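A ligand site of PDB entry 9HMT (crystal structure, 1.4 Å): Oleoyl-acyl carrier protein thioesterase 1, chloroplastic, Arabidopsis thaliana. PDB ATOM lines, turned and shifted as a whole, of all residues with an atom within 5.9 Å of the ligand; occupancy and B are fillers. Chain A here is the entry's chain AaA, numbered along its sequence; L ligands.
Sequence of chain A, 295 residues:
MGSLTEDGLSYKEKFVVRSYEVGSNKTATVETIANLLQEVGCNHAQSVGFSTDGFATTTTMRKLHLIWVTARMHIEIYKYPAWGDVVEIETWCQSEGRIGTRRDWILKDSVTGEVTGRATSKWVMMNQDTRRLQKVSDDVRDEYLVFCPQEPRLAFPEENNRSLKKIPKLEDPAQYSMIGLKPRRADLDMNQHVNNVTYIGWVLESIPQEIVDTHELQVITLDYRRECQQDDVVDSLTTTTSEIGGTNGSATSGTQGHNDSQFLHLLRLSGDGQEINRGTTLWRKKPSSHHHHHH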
ATOM      1  N   LEU A  37       5.102  38.496  -6.499  1.00  0.00           N
ATOM      2  CA  LEU A  37       5.091  37.015  -6.716  1.00  0.00           C
ATOM      3  C   LEU A  37       3.753  36.440  -6.281  1.00  0.00           C
ATOM      4  O   LEU A  37       3.144  35.599  -6.975  1.00  0.00           O
ATOM      5  CB  LEU A  37       6.233  36.352  -5.938  1.00  0.00           C
ATOM      6  CG  LEU A  37       7.656  36.763  -6.282  1.00  0.00           C
ATOM      7  CD1 LEU A  37       8.641  35.956  -5.474  1.00  0.00           C
ATOM      8  CD2 LEU A  37       7.966  36.638  -7.773  1.00  0.00           C
ATOM      9  N   GLN A  38       3.267  36.855  -5.118  1.00  0.00           N
ATOM     10  CA  GLN A  38       1.969  36.362  -4.609  1.00  0.00           C
ATOM     11  C   GLN A  38       0.849  36.764  -5.575  1.00  0.00           C
ATOM     12  O   GLN A  38      -0.029  35.948  -5.885  1.00  0.00           O
ATOM     13  CB  GLN A  38       1.599  36.940  -3.241  1.00  0.00           C
ATOM     14  CG  GLN A  38       0.249  36.443  -2.749  1.00  0.00           C
ATOM     15  CD  GLN A  38      -0.281  37.206  -1.579  1.00  0.00           C
ATOM     16  OE1 GLN A  38      -1.371  37.793  -1.633  1.00  0.00           O
ATOM     17  NE2 GLN A  38       0.508  37.215  -0.519  1.00  0.00           N
ATOM     18  N   VAL A  40       0.843  37.582  -8.817  1.00  0.00           N
ATOM     19  CA  VAL A  40       0.812  36.889 -10.138  1.00  0.00           C
ATOM     20  C   VAL A  40       0.404  35.429  -9.907  1.00  0.00           C
ATOM     21  O   VAL A  40      -0.308  34.856 -10.750  1.00  0.00           O
ATOM     22  CB  VAL A  40       2.118  37.043 -10.908  1.00  0.00           C
ATOM     23  CG1 VAL A  40       3.302  36.355 -10.255  1.00  0.00           C
ATOM     24  CG2 VAL A  40       1.952  36.597 -12.357  1.00  0.00           C
ATOM     25  N   GLY A  41       0.798  34.812  -8.798  1.00  0.00           N
ATOM     26  CA  GLY A  41       0.347  33.452  -8.467  1.00  0.00           C
ATOM     27  C   GLY A  41      -1.158  33.399  -8.316  1.00  0.00           C
ATOM     28  O   GLY A  41      -1.823  32.489  -8.864  1.00  0.00           O
ATOM     29  N   CYS A  42      -1.738  34.358  -7.599  1.00  0.00           N
ATOM     30  CA  CYS A  42      -3.195  34.424  -7.426  1.00  0.00           C
ATOM     31  C   CYS A  42      -3.906  34.655  -8.748  1.00  0.00           C
ATOM     32  O   CYS A  42      -4.981  34.061  -8.971  1.00  0.00           O
ATOM     33  CB  CYS A  42      -3.595  35.545  -6.481  1.00  0.00           C
ATOM     34  SG  CYS A  42      -3.219  35.193  -4.758  1.00  0.00           S
ATOM     35  N   HIS A  44      -2.764  33.820 -11.725  1.00  0.00           N
ATOM     36  CA  HIS A  44      -2.627  32.530 -12.438  1.00  0.00           C
ATOM     37  C   HIS A  44      -3.729  31.597 -11.973  1.00  0.00           C
ATOM     38  O   HIS A  44      -4.447  31.025 -12.844  1.00  0.00           O
ATOM     39  CB  HIS A  44      -1.259  31.942 -12.169  1.00  0.00           C
ATOM     40  CG  HIS A  44      -0.994  30.688 -12.931  1.00  0.00           C
ATOM     41  ND1 HIS A  44       0.024  29.847 -12.581  1.00  0.00           N
ATOM     42  CD2 HIS A  44      -1.643  30.115 -13.976  1.00  0.00           C
ATOM     43  CE1 HIS A  44       0.028  28.814 -13.415  1.00  0.00           C
ATOM     44  NE2 HIS A  44      -0.972  28.956 -14.294  1.00  0.00           N
ATOM     45  N   ALA A  45      -3.894  31.441 -10.676  1.00  0.00           N
ATOM     46  CA  ALA A  45      -4.921  30.537 -10.117  1.00  0.00           C
ATOM     47  C   ALA A  45      -6.279  30.933 -10.684  1.00  0.00           C
ATOM     48  O   ALA A  45      -7.051  30.058 -11.113  1.00  0.00           O
ATOM     49  CB  ALA A  45      -4.902  30.527  -8.622  1.00  0.00           C
ATOM     50  N   GLN A  46      -6.619  32.220 -10.680  1.00  0.00           N
ATOM     51  CA  GLN A  46      -7.966  32.597 -11.164  1.00  0.00           C
ATOM     52  C   GLN A  46      -8.088  32.287 -12.647  1.00  0.00           C
ATOM     53  O   GLN A  46      -9.208  31.902 -13.092  1.00  0.00           O
ATOM     54  CB  GLN A  46      -8.196  34.084 -10.916  1.00  0.00           C
ATOM     55  CG  GLN A  46      -8.405  34.296  -9.451  1.00  0.00           C
ATOM     56  CD  GLN A  46      -8.600  35.754  -9.111  1.00  0.00           C
ATOM     57  OE1 GLN A  46      -9.714  36.277  -9.147  1.00  0.00           O
ATOM     58  NE2 GLN A  46      -7.504  36.406  -8.810  1.00  0.00           N
ATOM     59  N   VAL A  48      -6.952  29.909 -14.369  1.00  0.00           N
ATOM     60  CA  VAL A  48      -7.178  28.466 -14.661  1.00  0.00           C
ATOM     61  C   VAL A  48      -8.356  27.945 -13.838  1.00  0.00           C
ATOM     62  O   VAL A  48      -8.559  26.727 -13.773  1.00  0.00           O
ATOM     63  CB  VAL A  48      -5.898  27.636 -14.447  1.00  0.00           C
ATOM     64  CG1 VAL A  48      -4.793  28.160 -15.333  1.00  0.00           C
ATOM     65  CG2 VAL A  48      -5.467  27.559 -12.994  1.00  0.00           C
ATOM     66  N   PHE A  50      -9.637  28.661 -10.697  1.00  0.00           N
ATOM     67  CA  PHE A  50      -9.780  28.737  -9.238  1.00  0.00           C
ATOM     68  C   PHE A  50     -10.612  29.989  -8.926  1.00  0.00           C
ATOM     69  O   PHE A  50     -10.897  30.868  -9.810  1.00  0.00           O
ATOM     70  CB  PHE A  50      -8.425  28.703  -8.533  1.00  0.00           C
ATOM     71  CG  PHE A  50      -7.691  27.384  -8.646  1.00  0.00           C
ATOM     72  CD1 PHE A  50      -7.961  26.347  -7.784  1.00  0.00           C
ATOM     73  CD2 PHE A  50      -6.772  27.175  -9.656  1.00  0.00           C
ATOM     74  CE1 PHE A  50      -7.297  25.128  -7.900  1.00  0.00           C
ATOM     75  CE2 PHE A  50      -6.096  25.963  -9.773  1.00  0.00           C
ATOM     76  CZ  PHE A  50      -6.361  24.938  -8.891  1.00  0.00           C
ATOM     77  N   PHE A  55      -8.482  32.234  -1.886  1.00  0.00           N
ATOM     78  CA  PHE A  55      -7.233  31.604  -2.360  1.00  0.00           C
ATOM     79  C   PHE A  55      -7.535  30.221  -2.938  1.00  0.00           C
ATOM     80  O   PHE A  55      -8.502  29.561  -2.513  1.00  0.00           O
ATOM     81  CB  PHE A  55      -6.196  31.516  -1.248  1.00  0.00           C
ATOM     82  CG  PHE A  55      -5.704  32.849  -0.764  1.00  0.00           C
ATOM     83  CD1 PHE A  55      -5.111  33.739  -1.642  1.00  0.00           C
ATOM     84  CD2 PHE A  55      -5.783  33.181   0.583  1.00  0.00           C
ATOM     85  CE1 PHE A  55      -4.617  34.950  -1.192  1.00  0.00           C
ATOM     86  CE2 PHE A  55      -5.290  34.405   1.027  1.00  0.00           C
ATOM     87  CZ  PHE A  55      -4.718  35.284   0.131  1.00  0.00           C
ATOM     88  N   ALA A  56      -6.730  29.836  -3.922  1.00  0.00           N
ATOM     89  CA  ALA A  56      -6.936  28.618  -4.739  1.00  0.00           C
ATOM     90  C   ALA A  56      -7.123  27.370  -3.861  1.00  0.00           C
ATOM     91  O   ALA A  56      -6.310  27.058  -2.969  1.00  0.00           O
ATOM     92  CB  ALA A  56      -5.788  28.464  -5.696  1.00  0.00           C
ATOM     93  N   THR A  58      -8.725  23.207  -4.843  1.00  0.00           N
ATOM     94  CA  THR A  58      -9.453  22.285  -5.754  1.00  0.00           C
ATOM     95  C   THR A  58     -10.761  21.855  -5.095  1.00  0.00           C
ATOM     96  O   THR A  58     -10.967  22.071  -3.863  1.00  0.00           O
ATOM     97  CB  THR A  58      -8.629  21.051  -6.136  1.00  0.00           C
ATOM     98  OG1 THR A  58      -8.589  20.166  -5.018  1.00  0.00           O
ATOM     99  CG2 THR A  58      -7.227  21.351  -6.595  1.00  0.00           C
ATOM    100  N   TRP A  68      -3.601  25.142   0.581  1.00  0.00           N
ATOM    101  CA  TRP A  68      -2.157  25.194   0.285  1.00  0.00           C
ATOM    102  C   TRP A  68      -1.524  26.221   1.220  1.00  0.00           C
ATOM    103  O   TRP A  68      -2.045  27.330   1.373  1.00  0.00           O
ATOM    104  CB  TRP A  68      -1.922  25.594  -1.178  1.00  0.00           C
ATOM    105  CG  TRP A  68      -1.855  24.487  -2.188  1.00  0.00           C
ATOM    106  CD1 TRP A  68      -0.915  23.501  -2.311  1.00  0.00           C
ATOM    107  CD2 TRP A  68      -2.761  24.311  -3.293  1.00  0.00           C
ATOM    108  NE1 TRP A  68      -1.171  22.735  -3.419  1.00  0.00           N
ATOM    109  CE2 TRP A  68      -2.277  23.220  -4.053  1.00  0.00           C
ATOM    110  CE3 TRP A  68      -3.874  25.005  -3.730  1.00  0.00           C
ATOM    111  CZ2 TRP A  68      -2.929  22.780  -5.209  1.00  0.00           C
ATOM    112  CZ3 TRP A  68      -4.525  24.573  -4.857  1.00  0.00           C
ATOM    113  CH2 TRP A  68      -4.059  23.479  -5.591  1.00  0.00           C
ATOM    114  N   TRP A  92       4.568  29.420 -12.928  1.00  0.00           N
ATOM    115  CA  TRP A  92       3.968  28.107 -13.215  1.00  0.00           C
ATOM    116  C   TRP A  92       4.065  27.269 -11.956  1.00  0.00           C
ATOM    117  O   TRP A  92       4.835  27.582 -11.032  1.00  0.00           O
ATOM    118  CB  TRP A  92       4.646  27.412 -14.407  1.00  0.00           C
ATOM    119  CG  TRP A  92       6.084  27.111 -14.208  1.00  0.00           C
ATOM    120  CD1 TRP A  92       6.614  25.924 -13.787  1.00  0.00           C
ATOM    121  CD2 TRP A  92       7.202  28.005 -14.375  1.00  0.00           C
ATOM    122  NE1 TRP A  92       7.964  26.029 -13.663  1.00  0.00           N
ATOM    123  CE2 TRP A  92       8.362  27.284 -14.037  1.00  0.00           C
ATOM    124  CE3 TRP A  92       7.351  29.332 -14.801  1.00  0.00           C
ATOM    125  CZ2 TRP A  92       9.640  27.823 -14.113  1.00  0.00           C
ATOM    126  CZ3 TRP A  92       8.613  29.861 -14.867  1.00  0.00           C
ATOM    127  CH2 TRP A  92       9.737  29.118 -14.522  1.00  0.00           C
ATOM    128  N   CYS A  93       3.316  26.183 -11.941  1.00  0.00           N
ATOM    129  CA  CYS A  93       3.358  25.212 -10.863  1.00  0.00           C
ATOM    130  C   CYS A  93       3.762  23.849 -11.390  1.00  0.00           C
ATOM    131  O   CYS A  93       3.525  23.562 -12.566  1.00  0.00           O
ATOM    132  CB  CYS A  93       2.000  25.056 -10.198  1.00  0.00           C
ATOM    133  SG  CYS A  93       1.408  26.555  -9.386  1.00  0.00           S
ATOM    134  N   THR A 101       3.244  20.892  -3.732  1.00  0.00           N
ATOM    135  CA  THR A 101       3.123  21.570  -5.021  1.00  0.00           C
ATOM    136  C   THR A 101       4.150  22.692  -5.051  1.00  0.00           C
ATOM    137  O   THR A 101       4.291  23.420  -4.049  1.00  0.00           O
ATOM    138  CB  THR A 101       1.705  22.107  -5.230  1.00  0.00           C
ATOM    139  OG1 THR A 101       0.750  21.116  -4.886  1.00  0.00           O
ATOM    140  CG2 THR A 101       1.484  22.626  -6.626  1.00  0.00           C
ATOM    141  N   ARG A 102       4.846  22.845  -6.145  1.00  0.00           N
ATOM    142  CA  ARG A 102       5.820  23.914  -6.317  1.00  0.00           C
ATOM    143  C   ARG A 102       5.209  25.024  -7.144  1.00  0.00           C
ATOM    144  O   ARG A 102       4.477  24.742  -8.118  1.00  0.00           O
ATOM    145  CB  ARG A 102       7.045  23.319  -7.024  1.00  0.00           C
ATOM    146  CG  ARG A 102       8.354  24.000  -6.704  1.00  0.00           C
ATOM    147  CD  ARG A 102       9.518  23.302  -7.357  1.00  0.00           C
ATOM    148  NE  ARG A 102       9.590  23.696  -8.727  1.00  0.00           N
ATOM    149  CZ  ARG A 102       9.422  22.944  -9.818  1.00  0.00           C
ATOM    150  NH1 ARG A 102       9.496  23.583 -10.955  1.00  0.00           N
ATOM    151  NH2 ARG A 102       9.194  21.639  -9.808  1.00  0.00           N
ATOM    152  N   ARG A 103       5.561  26.252  -6.800  1.00  0.00           N
ATOM    153  CA  ARG A 103       5.313  27.410  -7.689  1.00  0.00           C
ATOM    154  C   ARG A 103       6.648  28.072  -7.947  1.00  0.00           C
ATOM    155  O   ARG A 103       7.385  28.362  -7.003  1.00  0.00           O
ATOM    156  CB  ARG A 103       4.294  28.423  -7.150  1.00  0.00           C
ATOM    157  CG  ARG A 103       4.150  29.635  -8.067  1.00  0.00           C
ATOM    158  CD  ARG A 103       3.038  30.601  -7.726  1.00  0.00           C
ATOM    159  NE  ARG A 103       1.724  30.044  -7.888  1.00  0.00           N
ATOM    160  CZ  ARG A 103       1.081  29.947  -9.034  1.00  0.00           C
ATOM    161  NH1 ARG A 103      -0.131  29.450  -9.050  1.00  0.00           N
ATOM    162  NH2 ARG A 103       1.659  30.327 -10.145  1.00  0.00           N
ATOM    163  N   TRP A 105       8.838  31.147 -10.309  1.00  0.00           N
ATOM    164  CA  TRP A 105       8.682  32.441 -10.982  1.00  0.00           C
ATOM    165  C   TRP A 105       9.987  32.842 -11.619  1.00  0.00           C
ATOM    166  O   TRP A 105      11.060  32.607 -11.056  1.00  0.00           O
ATOM    167  CB  TRP A 105       8.289  33.537  -9.996  1.00  0.00           C
ATOM    168  CG  TRP A 105       7.049  33.439  -9.188  1.00  0.00           C
ATOM    169  CD1 TRP A 105       5.891  34.123  -9.368  1.00  0.00           C
ATOM    170  CD2 TRP A 105       6.910  32.785  -7.907  1.00  0.00           C
ATOM    171  NE1 TRP A 105       5.018  33.899  -8.333  1.00  0.00           N
ATOM    172  CE2 TRP A 105       5.635  33.093  -7.417  1.00  0.00           C
ATOM    173  CE3 TRP A 105       7.749  31.982  -7.140  1.00  0.00           C
ATOM    174  CZ2 TRP A 105       5.183  32.661  -6.176  1.00  0.00           C
ATOM    175  CZ3 TRP A 105       7.300  31.529  -5.908  1.00  0.00           C
ATOM    176  CH2 TRP A 105       6.035  31.882  -5.440  1.00  0.00           C
ATOM    177  N   TRP A 123       4.859  24.424  -1.487  1.00  0.00           N
ATOM    178  CA  TRP A 123       3.561  24.533  -0.796  1.00  0.00           C
ATOM    179  C   TRP A 123       3.133  23.149  -0.377  1.00  0.00           C
ATOM    180  O   TRP A 123       3.286  22.194  -1.154  1.00  0.00           O
ATOM    181  CB  TRP A 123       2.517  25.153  -1.677  1.00  0.00           C
ATOM    182  CG  TRP A 123       2.824  26.544  -2.135  1.00  0.00           C
ATOM    183  CD1 TRP A 123       3.746  26.910  -3.075  1.00  0.00           C
ATOM    184  CD2 TRP A 123       2.136  27.743  -1.769  1.00  0.00           C
ATOM    185  NE1 TRP A 123       3.718  28.259  -3.266  1.00  0.00           N
ATOM    186  CE2 TRP A 123       2.722  28.803  -2.495  1.00  0.00           C
ATOM    187  CE3 TRP A 123       1.096  28.042  -0.882  1.00  0.00           C
ATOM    188  CZ2 TRP A 123       2.303  30.130  -2.379  1.00  0.00           C
ATOM    189  CZ3 TRP A 123       0.675  29.358  -0.772  1.00  0.00           C
ATOM    190  CH2 TRP A 123       1.269  30.375  -1.501  1.00  0.00           C
ATOM    191  N   TYR A 144      -5.464  19.301 -10.157  1.00  0.00           N
ATOM    192  CA  TYR A 144      -4.602  20.443 -10.541  1.00  0.00           C
ATOM    193  C   TYR A 144      -3.516  20.086 -11.557  1.00  0.00           C
ATOM    194  O   TYR A 144      -2.945  20.996 -12.140  1.00  0.00           O
ATOM    195  CB  TYR A 144      -4.027  21.117  -9.302  1.00  0.00           C
ATOM    196  CG  TYR A 144      -2.819  20.493  -8.667  1.00  0.00           C
ATOM    197  CD1 TYR A 144      -1.555  20.686  -9.180  1.00  0.00           C
ATOM    198  CD2 TYR A 144      -2.926  19.822  -7.452  1.00  0.00           C
ATOM    199  CE1 TYR A 144      -0.436  20.163  -8.558  1.00  0.00           C
ATOM    200  CE2 TYR A 144      -1.812  19.296  -6.821  1.00  0.00           C
ATOM    201  CZ  TYR A 144      -0.557  19.478  -7.369  1.00  0.00           C
ATOM    202  OH  TYR A 144       0.585  19.064  -6.755  1.00  0.00           O
ATOM    203  N   PHE A 147      -3.117  21.697 -15.045  1.00  0.00           N
ATOM    204  CA  PHE A 147      -2.710  23.102 -15.156  1.00  0.00           C
ATOM    205  C   PHE A 147      -1.198  23.285 -15.078  1.00  0.00           C
ATOM    206  O   PHE A 147      -0.740  24.429 -15.064  1.00  0.00           O
ATOM    207  CB  PHE A 147      -3.391  23.930 -14.073  1.00  0.00           C
ATOM    208  CG  PHE A 147      -4.882  23.769 -14.068  1.00  0.00           C
ATOM    209  CD1 PHE A 147      -5.647  23.996 -15.197  1.00  0.00           C
ATOM    210  CD2 PHE A 147      -5.533  23.341 -12.921  1.00  0.00           C
ATOM    211  CE1 PHE A 147      -7.013  23.787 -15.169  1.00  0.00           C
ATOM    212  CE2 PHE A 147      -6.901  23.165 -12.892  1.00  0.00           C
ATOM    213  CZ  PHE A 147      -7.634  23.366 -14.029  1.00  0.00           C
ATOM    214  N   CYS A 148      -0.458  22.187 -15.017  1.00  0.00           N
ATOM    215  CA  CYS A 148       1.003  22.200 -14.790  1.00  0.00           C
ATOM    216  C   CYS A 148       1.726  21.586 -15.968  1.00  0.00           C
ATOM    217  O   CYS A 148       1.308  20.552 -16.515  1.00  0.00           O
ATOM    218  CB  CYS A 148       1.363  21.371 -13.581  1.00  0.00           C
ATOM    219  SG  CYS A 148       0.595  21.923 -12.048  1.00  0.00           S
HETATM  220  C1  LIG L   1       0.538  25.824  -4.873  1.00  0.00           C
HETATM  221  F1  LIG L   1      -2.447  24.020  -8.498  1.00  0.00           F
HETATM  222  N1  LIG L   1       0.187  29.103  -5.780  1.00  0.00           N
HETATM  223  O1  LIG L   1      -2.204  27.220  -6.995  1.00  0.00           O
HETATM  224  C2  LIG L   1      -0.395  26.848  -5.459  1.00  0.00           C
HETATM  225  O2  LIG L   1       0.455  27.785  -6.211  1.00  0.00           O
HETATM  226  C3  LIG L   1      -1.349  26.227  -6.448  1.00  0.00           C
HETATM  227  C4  LIG L   1      -3.219  26.665  -7.823  1.00  0.00           C
HETATM  228  C5  LIG L   1      -2.646  26.272  -9.163  1.00  0.00           C
HETATM  229  C6  LIG L   1      -2.255  24.954  -9.439  1.00  0.00           C
HETATM  230  C7  LIG L   1      -1.741  24.586 -10.650  1.00  0.00           C
HETATM  231  C8  LIG L   1      -1.536  25.544 -11.623  1.00  0.00           C
HETATM  232  C9  LIG L   1      -1.892  26.844 -11.398  1.00  0.00           C
HETATM  233  C10 LIG L   1      -2.434  27.193 -10.174  1.00  0.00           C
HETATM  234  C11 LIG L   1      -1.069  27.710  -4.407  1.00  0.00           C
HETATM  235  C12 LIG L   1      -0.630  29.085  -4.800  1.00  0.00           C
HETATM  236  C13 LIG L   1      -1.011  30.316  -4.101  1.00  0.00           C
HETATM  237  C14 LIG L   1      -1.927  30.262  -3.043  1.00  0.00           C
HETATM  238  C15 LIG L   1      -2.307  31.416  -2.369  1.00  0.00           C
HETATM  239  C16 LIG L   1      -1.759  32.639  -2.726  1.00  0.00           C
HETATM  240  C17 LIG L   1      -0.856  32.710  -3.795  1.00  0.00           C
HETATM  241  C18 LIG L   1      -0.490  31.557  -4.452  1.00  0.00           C
HETATM  242  F2  LIG L   1       0.401  31.661  -5.473  1.00  0.00           F
HETATM  243  F3  LIG L   1      -2.751  28.502  -9.936  1.00  0.00           F
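O2 of the ligand sits at hydrogen-bond distance from SG of Cys 93 (3.5 Å).
N1 of the ligand sits at hydrogen-bond distance from NE of Arg 103, 2.8 Å away.
NH1 of Arg 103 sits at hydrogen-bond distance from SG of Cys 93, at 3.3 Å.
The side-chain sulfur (SG) of Cys 42 sits at hydrogen-bond distance from the backbone carbonyl oxygen (O) of Gln 38.
The backbone carbonyl oxygen of Tyr 144 lies within hydrogen-bond range of the side-chain sulfur of Cys 148 (3.7 Å).
The guanidinium group (NH1) of Arg 103 is in hydrogen-bond range of the backbone carbonyl oxygen (O) of Gly 41.
The indole nitrogen (NE1) of Trp 68 sits at hydrogen-bond distance from the side-chain hydroxyl (OG1) of Thr 101.
A ring nitrogen (ND1) of His 44 lies within hydrogen-bond range of the guanidinium group of Arg 103, at 3.0 Å.
The backbone carbonyl oxygen of Thr 101 is in hydrogen-bond range of the backbone NH of Trp 123 (2.8 Å).
O of Ala 45 lies within hydrogen-bond range of N of Phe 50.
The backbone NH of Ala 45 sits close to a fluorine (F3) of the ligand (3.2 Å).
Residues that only touch the ligand: Gln 38 (3.9 Å), Gly 41 (3.5 Å), Cys 42 (3.6 Å), His 44 (3.4 Å), Val 48 (3.98 Å), Phe 50 (3.5 Å), Phe 55 (3.7 Å), Ala 56 (3.8 Å), Trp 68 (3.4 Å), Thr 101 (3.8 Å), Trp 123 (3.5 Å), Tyr 144 (3.4 Å), Phe 147 (3.5 Å) and Cys 148 (3.8 Å).
Within 4 Å of the ligand: Gln 38, Gly 41, Cys 42, His 44, Ala 45, Val 48, Phe 50, Phe 55, Ala 56, Trp 68, Cys 93, Thr 101, Arg 103, Trp 123, Tyr 144, Phe 147 and Cys 148.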
